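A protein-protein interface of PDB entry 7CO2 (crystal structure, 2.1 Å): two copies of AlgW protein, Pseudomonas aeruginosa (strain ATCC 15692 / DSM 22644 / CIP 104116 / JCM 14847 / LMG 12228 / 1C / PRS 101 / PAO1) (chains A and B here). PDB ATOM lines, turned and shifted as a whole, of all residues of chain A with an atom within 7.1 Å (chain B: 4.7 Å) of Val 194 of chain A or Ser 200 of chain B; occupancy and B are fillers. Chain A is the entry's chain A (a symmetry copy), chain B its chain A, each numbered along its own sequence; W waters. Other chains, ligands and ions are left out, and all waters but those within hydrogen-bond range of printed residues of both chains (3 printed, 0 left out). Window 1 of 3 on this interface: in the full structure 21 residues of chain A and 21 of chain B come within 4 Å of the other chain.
The backbone carbonyl oxygen (O) of Val 194 of chain A is in hydrogen-bond range of the side-chain hydroxyl (OG) of Ser 200 of chain B, 2.6 Å away.
The side-chain amide nitrogen (NE2) of Gln 217 of chain B is in hydrogen-bond range of the side-chain hydroxyl (OG1) of Thr 193 of chain A, at 3.0 Å.
OD2 of Asp 219 of chain B is in hydrogen-bond range of N of Met 196 of chain A.
No position is printed for both chains.
Of the 11 pairs that touch across the chains among the printed residues, none has its exchanged pair printed and touching as well.
Val 59 of chain A touches Thr 177 of chain B.
Gln 192 of chain A touches Ala 201 of chain B (O to CB, 3.9 Å).
CA of Thr 193 of chain A touches O of Ser 200 of chain B, 3.7 Å away.
CG2 of Val 194 of chain A touches CG2 of Thr 177 of chain B (3.6 Å).
Val 194 of chain A touches Ile 198 of chain B (O to CD1, 3.6 Å).
Thr 195 of chain A touches Ile 198 of chain B (C to CD1, 3.9 Å).
CA of Thr 195 of chain A touches OD2 of Asp 219 of chain B, 3.4 Å away.
Ile 198 of chain B touches Met 196 of chain A.
Of the printed residues of chain B, Val 59 of chain A touches Thr 177 (3.6 Å).
Of the printed residues of chain B, Gln 192 of chain A touches Ala 201.
Of chain B, only Thr 177 (3.6 Å), Ile 198 (3.6 Å) and Ser 200 (2.6 Å) come within 4 Å of Val 194 of chain A.
Of the printed residues of chain B, Thr 195 of chain A touches Ile 198 and Asp 219.
Printed residues of chain A within 4 Å of Ile 198 of chain B: Val 194 (3.6 Å), Thr 195 (3.9 Å) and Met 196 (3.6 Å).
Of the printed residues of chain A, Asp 219 of chain B touches Thr 195 and Met 196.
The nearest printed residue of chain A that does not touch Ile 198 of chain B is Tyr 55 of chain A (4.2 Å).
Printed residues of chain B that touch a printed residue of chain A: Thr 177, Ile 198, Ser 200, Ala 201, Gln 217 and Asp 219.
Hydrophobic or aromatic side chains of chain A within 4 Å of the printed part of chain B: Val 59, Val 194 and Met 196.
Along chain A the printed residues that touch a printed residue of chain B span positions 59 to 196.
Among the printed residues, 11 pairs touch across the chains.
Among the printed residues, no Asp or Glu carboxylate lies within 4 Å of a Lys or Arg side-chain nitrogen of the other chain.
Water W2 bridges O of Met 196 of chain A and OD2 of Asp 219 of chain B.
Water W3 lies within hydrogen-bond range of the side-chain carboxylate (OD2) of Asp 219 of chain B (2.7 Å), the backbone carbonyl oxygen (O) of Met 196 of chain A (3.0 Å) and the backbone NH (N) of Ala 221 of chain A (3.1 Å).
Water W1 lies within hydrogen-bond range of O of Gln 192 of chain A (2.8 Å) and O of Ser 200 of chain B (3.0 Å).
O of Ile 198 of chain B is in hydrogen-bond range of OG1 of Thr 218 of chain B (2.8 Å).
The backbone NH (N) of Ser 200 of chain B is in hydrogen-bond range of the backbone carbonyl oxygen (O) of Gln 217 of chain B, at 2.6 Å.
O of Ala 63 of chain A sits at hydrogen-bond distance from NE2 of Gln 192 of chain A.
N of Ala 183 of chain A sits at hydrogen-bond distance from O of Thr 195 of chain A, 2.8 Å away.
The backbone carbonyl oxygen (O) of Gly 191 of chain A is in hydrogen-bond range of the side-chain hydroxyl (OG1) of Thr 193 of chain A, 2.8 Å away.
OG1 of Thr 195 of chain A is in hydrogen-bond range of O of Ala 221 of chain A (2.7 Å).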
ATOM      1  N   TYR A  55     -10.221  26.851   2.029  1.00  0.00           N
ATOM      2  CA  TYR A  55     -11.055  25.737   2.459  1.00  0.00           C
ATOM      3  C   TYR A  55     -11.710  25.026   1.282  1.00  0.00           C
ATOM      4  O   TYR A  55     -12.598  24.196   1.485  1.00  0.00           O
ATOM      5  CB  TYR A  55     -12.091  26.222   3.494  1.00  0.00           C
ATOM      6  CG  TYR A  55     -11.394  26.868   4.674  1.00  0.00           C
ATOM      7  CD1 TYR A  55     -10.851  26.102   5.705  1.00  0.00           C
ATOM      8  CD2 TYR A  55     -11.196  28.250   4.712  1.00  0.00           C
ATOM      9  CE1 TYR A  55     -10.168  26.706   6.775  1.00  0.00           C
ATOM     10  CE2 TYR A  55     -10.525  28.852   5.761  1.00  0.00           C
ATOM     11  CZ  TYR A  55     -10.018  28.080   6.788  1.00  0.00           C
ATOM     12  OH  TYR A  55      -9.359  28.744   7.789  1.00  0.00           O
ATOM     13  N   VAL A  59     -14.660  22.121   0.920  1.00  0.00           N
ATOM     14  CA  VAL A  59     -15.899  22.331   0.178  1.00  0.00           C
ATOM     15  C   VAL A  59     -16.090  21.240  -0.873  1.00  0.00           C
ATOM     16  O   VAL A  59     -17.194  20.707  -1.062  1.00  0.00           O
ATOM     17  CB  VAL A  59     -15.888  23.735  -0.439  1.00  0.00           C
ATOM     18  CG1 VAL A  59     -16.942  23.859  -1.583  1.00  0.00           C
ATOM     19  CG2 VAL A  59     -16.064  24.784   0.662  1.00  0.00           C
ATOM     20  N   ALA A  63     -19.624  19.515  -0.044  1.00  0.00           N
ATOM     21  CA  ALA A  63     -20.755  20.134  -0.718  1.00  0.00           C
ATOM     22  C   ALA A  63     -21.547  19.148  -1.574  1.00  0.00           C
ATOM     23  O   ALA A  63     -22.786  19.275  -1.624  1.00  0.00           O
ATOM     24  CB  ALA A  63     -20.248  21.305  -1.556  1.00  0.00           C
ATOM     25  N   CYS A 181     -14.865  26.179  11.109  1.00  0.00           N
ATOM     26  CA  CYS A 181     -15.925  25.339  10.569  1.00  0.00           C
ATOM     27  C   CYS A 181     -16.575  26.045   9.388  1.00  0.00           C
ATOM     28  O   CYS A 181     -16.405  27.248   9.181  1.00  0.00           O
ATOM     29  CB  CYS A 181     -16.980  24.988  11.593  1.00  0.00           C
ATOM     30  SG  CYS A 181     -17.661  26.436  12.370  1.00  0.00           S
ATOM     31  N   LEU A 182     -17.311  25.264   8.603  1.00  0.00           N
ATOM     32  CA  LEU A 182     -17.963  25.724   7.391  1.00  0.00           C
ATOM     33  C   LEU A 182     -19.422  25.322   7.451  1.00  0.00           C
ATOM     34  O   LEU A 182     -19.740  24.196   7.851  1.00  0.00           O
ATOM     35  CB  LEU A 182     -17.292  25.119   6.164  1.00  0.00           C
ATOM     36  CG  LEU A 182     -15.892  25.687   5.910  1.00  0.00           C
ATOM     37  CD1 LEU A 182     -14.939  25.363   7.026  1.00  0.00           C
ATOM     38  CD2 LEU A 182     -15.410  25.038   4.680  1.00  0.00           C
ATOM     39  N   ALA A 183     -20.306  26.248   7.095  1.00  0.00           N
ATOM     40  CA  ALA A 183     -21.737  25.978   7.009  1.00  0.00           C
ATOM     41  C   ALA A 183     -22.138  25.919   5.531  1.00  0.00           C
ATOM     42  O   ALA A 183     -21.698  26.762   4.740  1.00  0.00           O
ATOM     43  CB  ALA A 183     -22.529  27.057   7.749  1.00  0.00           C
ATOM     44  N   ILE A 184     -22.925  24.903   5.160  1.00  0.00           N
ATOM     45  CA  ILE A 184     -23.316  24.636   3.771  1.00  0.00           C
ATOM     46  C   ILE A 184     -24.844  24.512   3.707  1.00  0.00           C
ATOM     47  O   ILE A 184     -25.432  23.668   4.388  1.00  0.00           O
ATOM     48  CB  ILE A 184     -22.660  23.371   3.201  1.00  0.00           C
ATOM     49  CG1 ILE A 184     -21.165  23.309   3.564  1.00  0.00           C
ATOM     50  CG2 ILE A 184     -22.752  23.394   1.712  1.00  0.00           C
ATOM     51  CD1 ILE A 184     -20.387  22.148   2.941  1.00  0.00           C
ATOM     52  N   GLY A 185     -25.487  25.357   2.914  1.00  0.00           N
ATOM     53  CA  GLY A 185     -26.924  25.435   2.988  1.00  0.00           C
ATOM     54  C   GLY A 185     -27.454  26.236   1.838  1.00  0.00           C
ATOM     55  O   GLY A 185     -26.720  26.539   0.892  1.00  0.00           O
ATOM     56  N   PRO A 187     -29.213  29.594   2.000  1.00  0.00           N
ATOM     57  CA  PRO A 187     -29.792  30.765   2.689  1.00  0.00           C
ATOM     58  C   PRO A 187     -30.580  31.619   1.718  1.00  0.00           C
ATOM     59  O   PRO A 187     -30.128  31.891   0.606  1.00  0.00           O
ATOM     60  CB  PRO A 187     -28.571  31.511   3.252  1.00  0.00           C
ATOM     61  CG  PRO A 187     -27.445  31.053   2.446  1.00  0.00           C
ATOM     62  CD  PRO A 187     -27.748  29.704   1.887  1.00  0.00           C
ATOM     63  N   GLY A 191     -29.287  29.651  -3.485  1.00  0.00           N
ATOM     64  CA  GLY A 191     -28.459  28.590  -3.999  1.00  0.00           C
ATOM     65  C   GLY A 191     -27.521  28.077  -2.931  1.00  0.00           C
ATOM     66  O   GLY A 191     -27.293  28.712  -1.907  1.00  0.00           O
ATOM     67  N   GLN A 192     -26.991  26.884  -3.183  1.00  0.00           N
ATOM     68  CA  GLN A 192     -26.009  26.322  -2.274  1.00  0.00           C
ATOM     69  C   GLN A 192     -24.935  27.348  -1.982  1.00  0.00           C
ATOM     70  O   GLN A 192     -24.389  27.973  -2.891  1.00  0.00           O
ATOM     71  CB  GLN A 192     -25.385  25.059  -2.835  1.00  0.00           C
ATOM     72  CG  GLN A 192     -24.947  24.199  -1.665  1.00  0.00           C
ATOM     73  CD  GLN A 192     -24.023  23.097  -2.065  1.00  0.00           C
ATOM     74  OE1 GLN A 192     -22.997  23.325  -2.712  1.00  0.00           O
ATOM     75  NE2 GLN A 192     -24.363  21.892  -1.666  1.00  0.00           N
ATOM     76  N   THR A 193     -24.672  27.539  -0.703  1.00  0.00           N
ATOM     77  CA  THR A 193     -23.839  28.598  -0.168  1.00  0.00           C
ATOM     78  C   THR A 193     -22.930  28.027   0.894  1.00  0.00           C
ATOM     79  O   THR A 193     -23.390  27.296   1.775  1.00  0.00           O
ATOM     80  CB  THR A 193     -24.707  29.682   0.455  1.00  0.00           C
ATOM     81  OG1 THR A 193     -25.445  30.313  -0.585  1.00  0.00           O
ATOM     82  CG2 THR A 193     -23.828  30.758   1.145  1.00  0.00           C
ATOM     83  N   VAL A 194     -21.647  28.354   0.818  1.00  0.00           N
ATOM     84  CA  VAL A 194     -20.696  28.011   1.876  1.00  0.00           C
ATOM     85  C   VAL A 194     -20.336  29.285   2.662  1.00  0.00           C
ATOM     86  O   VAL A 194     -19.925  30.291   2.070  1.00  0.00           O
ATOM     87  CB  VAL A 194     -19.437  27.348   1.291  1.00  0.00           C
ATOM     88  CG1 VAL A 194     -18.452  26.859   2.452  1.00  0.00           C
ATOM     89  CG2 VAL A 194     -19.839  26.178   0.402  1.00  0.00           C
ATOM     90  N   THR A 195     -20.496  29.245   3.984  1.00  0.00           N
ATOM     91  CA  THR A 195     -20.044  30.303   4.884  1.00  0.00           C
ATOM     92  C   THR A 195     -19.017  29.765   5.861  1.00  0.00           C
ATOM     93  O   THR A 195     -19.001  28.578   6.165  1.00  0.00           O
ATOM     94  CB  THR A 195     -21.201  30.926   5.654  1.00  0.00           C
ATOM     95  OG1 THR A 195     -21.968  29.924   6.309  1.00  0.00           O
ATOM     96  CG2 THR A 195     -22.079  31.658   4.686  1.00  0.00           C
ATOM     97  N   MET A 196     -18.131  30.646   6.333  1.00  0.00           N
ATOM     98  CA  MET A 196     -17.003  30.223   7.152  1.00  0.00           C
ATOM     99  C   MET A 196     -17.035  30.926   8.498  1.00  0.00           C
ATOM    100  O   MET A 196     -17.296  32.122   8.564  1.00  0.00           O
ATOM    101  CB  MET A 196     -15.688  30.516   6.443  1.00  0.00           C
ATOM    102  CG  MET A 196     -14.463  29.896   7.057  1.00  0.00           C
ATOM    103  SD  MET A 196     -13.646  30.999   8.228  1.00  0.00           S
ATOM    104  CE  MET A 196     -13.147  32.335   7.134  1.00  0.00           C
ATOM    105  N   ALA A 221     -21.900  32.546   9.092  1.00  0.00           N
ATOM    106  CA  ALA A 221     -23.193  33.124   8.726  1.00  0.00           C
ATOM    107  C   ALA A 221     -24.205  32.030   8.392  1.00  0.00           C
ATOM    108  O   ALA A 221     -24.001  31.215   7.467  1.00  0.00           O
ATOM    109  CB  ALA A 221     -23.030  34.084   7.538  1.00  0.00           C
ATOM    110  N   ASN A 226     -30.867  27.867   5.706  1.00  0.00           N
ATOM    111  CA  ASN A 226     -29.747  27.023   6.098  1.00  0.00           C
ATOM    112  C   ASN A 226     -30.168  25.787   6.871  1.00  0.00           C
ATOM    113  O   ASN A 226     -29.324  24.920   7.114  1.00  0.00           O
ATOM    114  CB  ASN A 226     -28.726  27.788   6.948  1.00  0.00           C
ATOM    115  CG  ASN A 226     -27.634  28.448   6.116  1.00  0.00           C
ATOM    116  OD1 ASN A 226     -27.619  29.676   5.978  1.00  0.00           O
ATOM    117  ND2 ASN A 226     -26.690  27.659   5.620  1.00  0.00           N
ATOM    118  N   THR B 177     -14.839  28.084  -4.577  1.00  0.00           N
ATOM    119  CA  THR B 177     -15.581  28.165  -3.340  1.00  0.00           C
ATOM    120  C   THR B 177     -14.725  27.650  -2.198  1.00  0.00           C
ATOM    121  O   THR B 177     -14.015  26.649  -2.333  1.00  0.00           O
ATOM    122  CB  THR B 177     -16.864  27.361  -3.484  1.00  0.00           C
ATOM    123  OG1 THR B 177     -17.603  27.950  -4.548  1.00  0.00           O
ATOM    124  CG2 THR B 177     -17.703  27.363  -2.201  1.00  0.00           C
ATOM    125  N   ILE B 198     -14.967  34.062   2.902  1.00  0.00           N
ATOM    126  CA  ILE B 198     -14.616  33.086   1.880  1.00  0.00           C
ATOM    127  C   ILE B 198     -15.481  33.338   0.651  1.00  0.00           C
ATOM    128  O   ILE B 198     -16.487  34.051   0.710  1.00  0.00           O
ATOM    129  CB  ILE B 198     -14.788  31.611   2.330  1.00  0.00           C
ATOM    130  CG1 ILE B 198     -16.220  31.318   2.759  1.00  0.00           C
ATOM    131  CG2 ILE B 198     -13.853  31.271   3.450  1.00  0.00           C
ATOM    132  CD1 ILE B 198     -16.504  29.838   2.933  1.00  0.00           C
ATOM    133  N   ILE B 199     -15.069  32.758  -0.477  1.00  0.00           N
ATOM    134  CA  ILE B 199     -15.947  32.673  -1.646  1.00  0.00           C
ATOM    135  C   ILE B 199     -17.067  31.721  -1.251  1.00  0.00           C
ATOM    136  O   ILE B 199     -16.800  30.551  -0.942  1.00  0.00           O
ATOM    137  CB  ILE B 199     -15.202  32.156  -2.884  1.00  0.00           C
ATOM    138  CG1 ILE B 199     -13.954  32.979  -3.172  1.00  0.00           C
ATOM    139  CG2 ILE B 199     -16.104  32.141  -4.107  1.00  0.00           C
ATOM    140  CD1 ILE B 199     -14.216  34.438  -3.206  1.00  0.00           C
ATOM    141  N   SER B 200     -18.317  32.206  -1.264  1.00  0.00           N
ATOM    142  CA  SER B 200     -19.448  31.358  -0.873  1.00  0.00           C
ATOM    143  C   SER B 200     -19.998  30.563  -2.044  1.00  0.00           C
ATOM    144  O   SER B 200     -20.673  29.537  -1.849  1.00  0.00           O
ATOM    145  CB  SER B 200     -20.558  32.196  -0.252  1.00  0.00           C
ATOM    146  OG  SER B 200     -20.129  32.664   1.009  1.00  0.00           O
ATOM    147  N   ALA B 201     -19.725  31.007  -3.256  1.00  0.00           N
ATOM    148  CA  ALA B 201     -20.324  30.501  -4.484  1.00  0.00           C
ATOM    149  C   ALA B 201     -19.814  31.375  -5.623  1.00  0.00           C
ATOM    150  O   ALA B 201     -19.474  32.549  -5.424  1.00  0.00           O
ATOM    151  CB  ALA B 201     -21.849  30.539  -4.453  1.00  0.00           C
ATOM    152  N   GLN B 217     -20.128  35.213  -4.935  1.00  0.00           N
ATOM    153  CA  GLN B 217     -20.797  35.412  -3.654  1.00  0.00           C
ATOM    154  C   GLN B 217     -19.762  35.309  -2.536  1.00  0.00           C
ATOM    155  O   GLN B 217     -18.919  34.395  -2.534  1.00  0.00           O
ATOM    156  CB  GLN B 217     -21.927  34.379  -3.459  1.00  0.00           C
ATOM    157  CG  GLN B 217     -22.926  34.662  -2.328  1.00  0.00           C
ATOM    158  CD  GLN B 217     -23.932  33.526  -2.146  1.00  0.00           C
ATOM    159  OE1 GLN B 217     -24.560  33.099  -3.110  1.00  0.00           O
ATOM    160  NE2 GLN B 217     -24.070  33.014  -0.917  1.00  0.00           N
ATOM    161  N   THR B 218     -19.801  36.243  -1.594  1.00  0.00           N
ATOM    162  CA  THR B 218     -18.883  36.099  -0.475  1.00  0.00           C
ATOM    163  C   THR B 218     -19.580  36.334   0.845  1.00  0.00           C
ATOM    164  O   THR B 218     -20.574  37.051   0.904  1.00  0.00           O
ATOM    165  CB  THR B 218     -17.726  37.046  -0.513  1.00  0.00           C
ATOM    166  OG1 THR B 218     -17.018  36.839   0.705  1.00  0.00           O
ATOM    167  CG2 THR B 218     -18.214  38.474  -0.574  1.00  0.00           C
ATOM    168  N   ASP B 219     -19.034  35.744   1.917  1.00  0.00           N
ATOM    169  CA  ASP B 219     -19.526  36.086   3.234  1.00  0.00           C
ATOM    170  C   ASP B 219     -18.651  37.116   3.953  1.00  0.00           C
ATOM    171  O   ASP B 219     -18.954  37.448   5.100  1.00  0.00           O
ATOM    172  CB  ASP B 219     -19.752  34.842   4.117  1.00  0.00           C
ATOM    173  CG  ASP B 219     -18.471  34.167   4.528  1.00  0.00           C
ATOM    174  OD1 ASP B 219     -17.425  34.500   3.952  1.00  0.00           O
ATOM    175  OD2 ASP B 219     -18.514  33.293   5.436  1.00  0.00           O
HETATM  176  O   HOH W   1     -21.768  27.143  -3.314  1.00  0.00           O
HETATM  177  O   HOH W   2     -16.388  33.842   6.933  1.00  0.00           O
HETATM  178  O   HOH W   3     -19.514  33.971   7.835  1.00  0.00           O
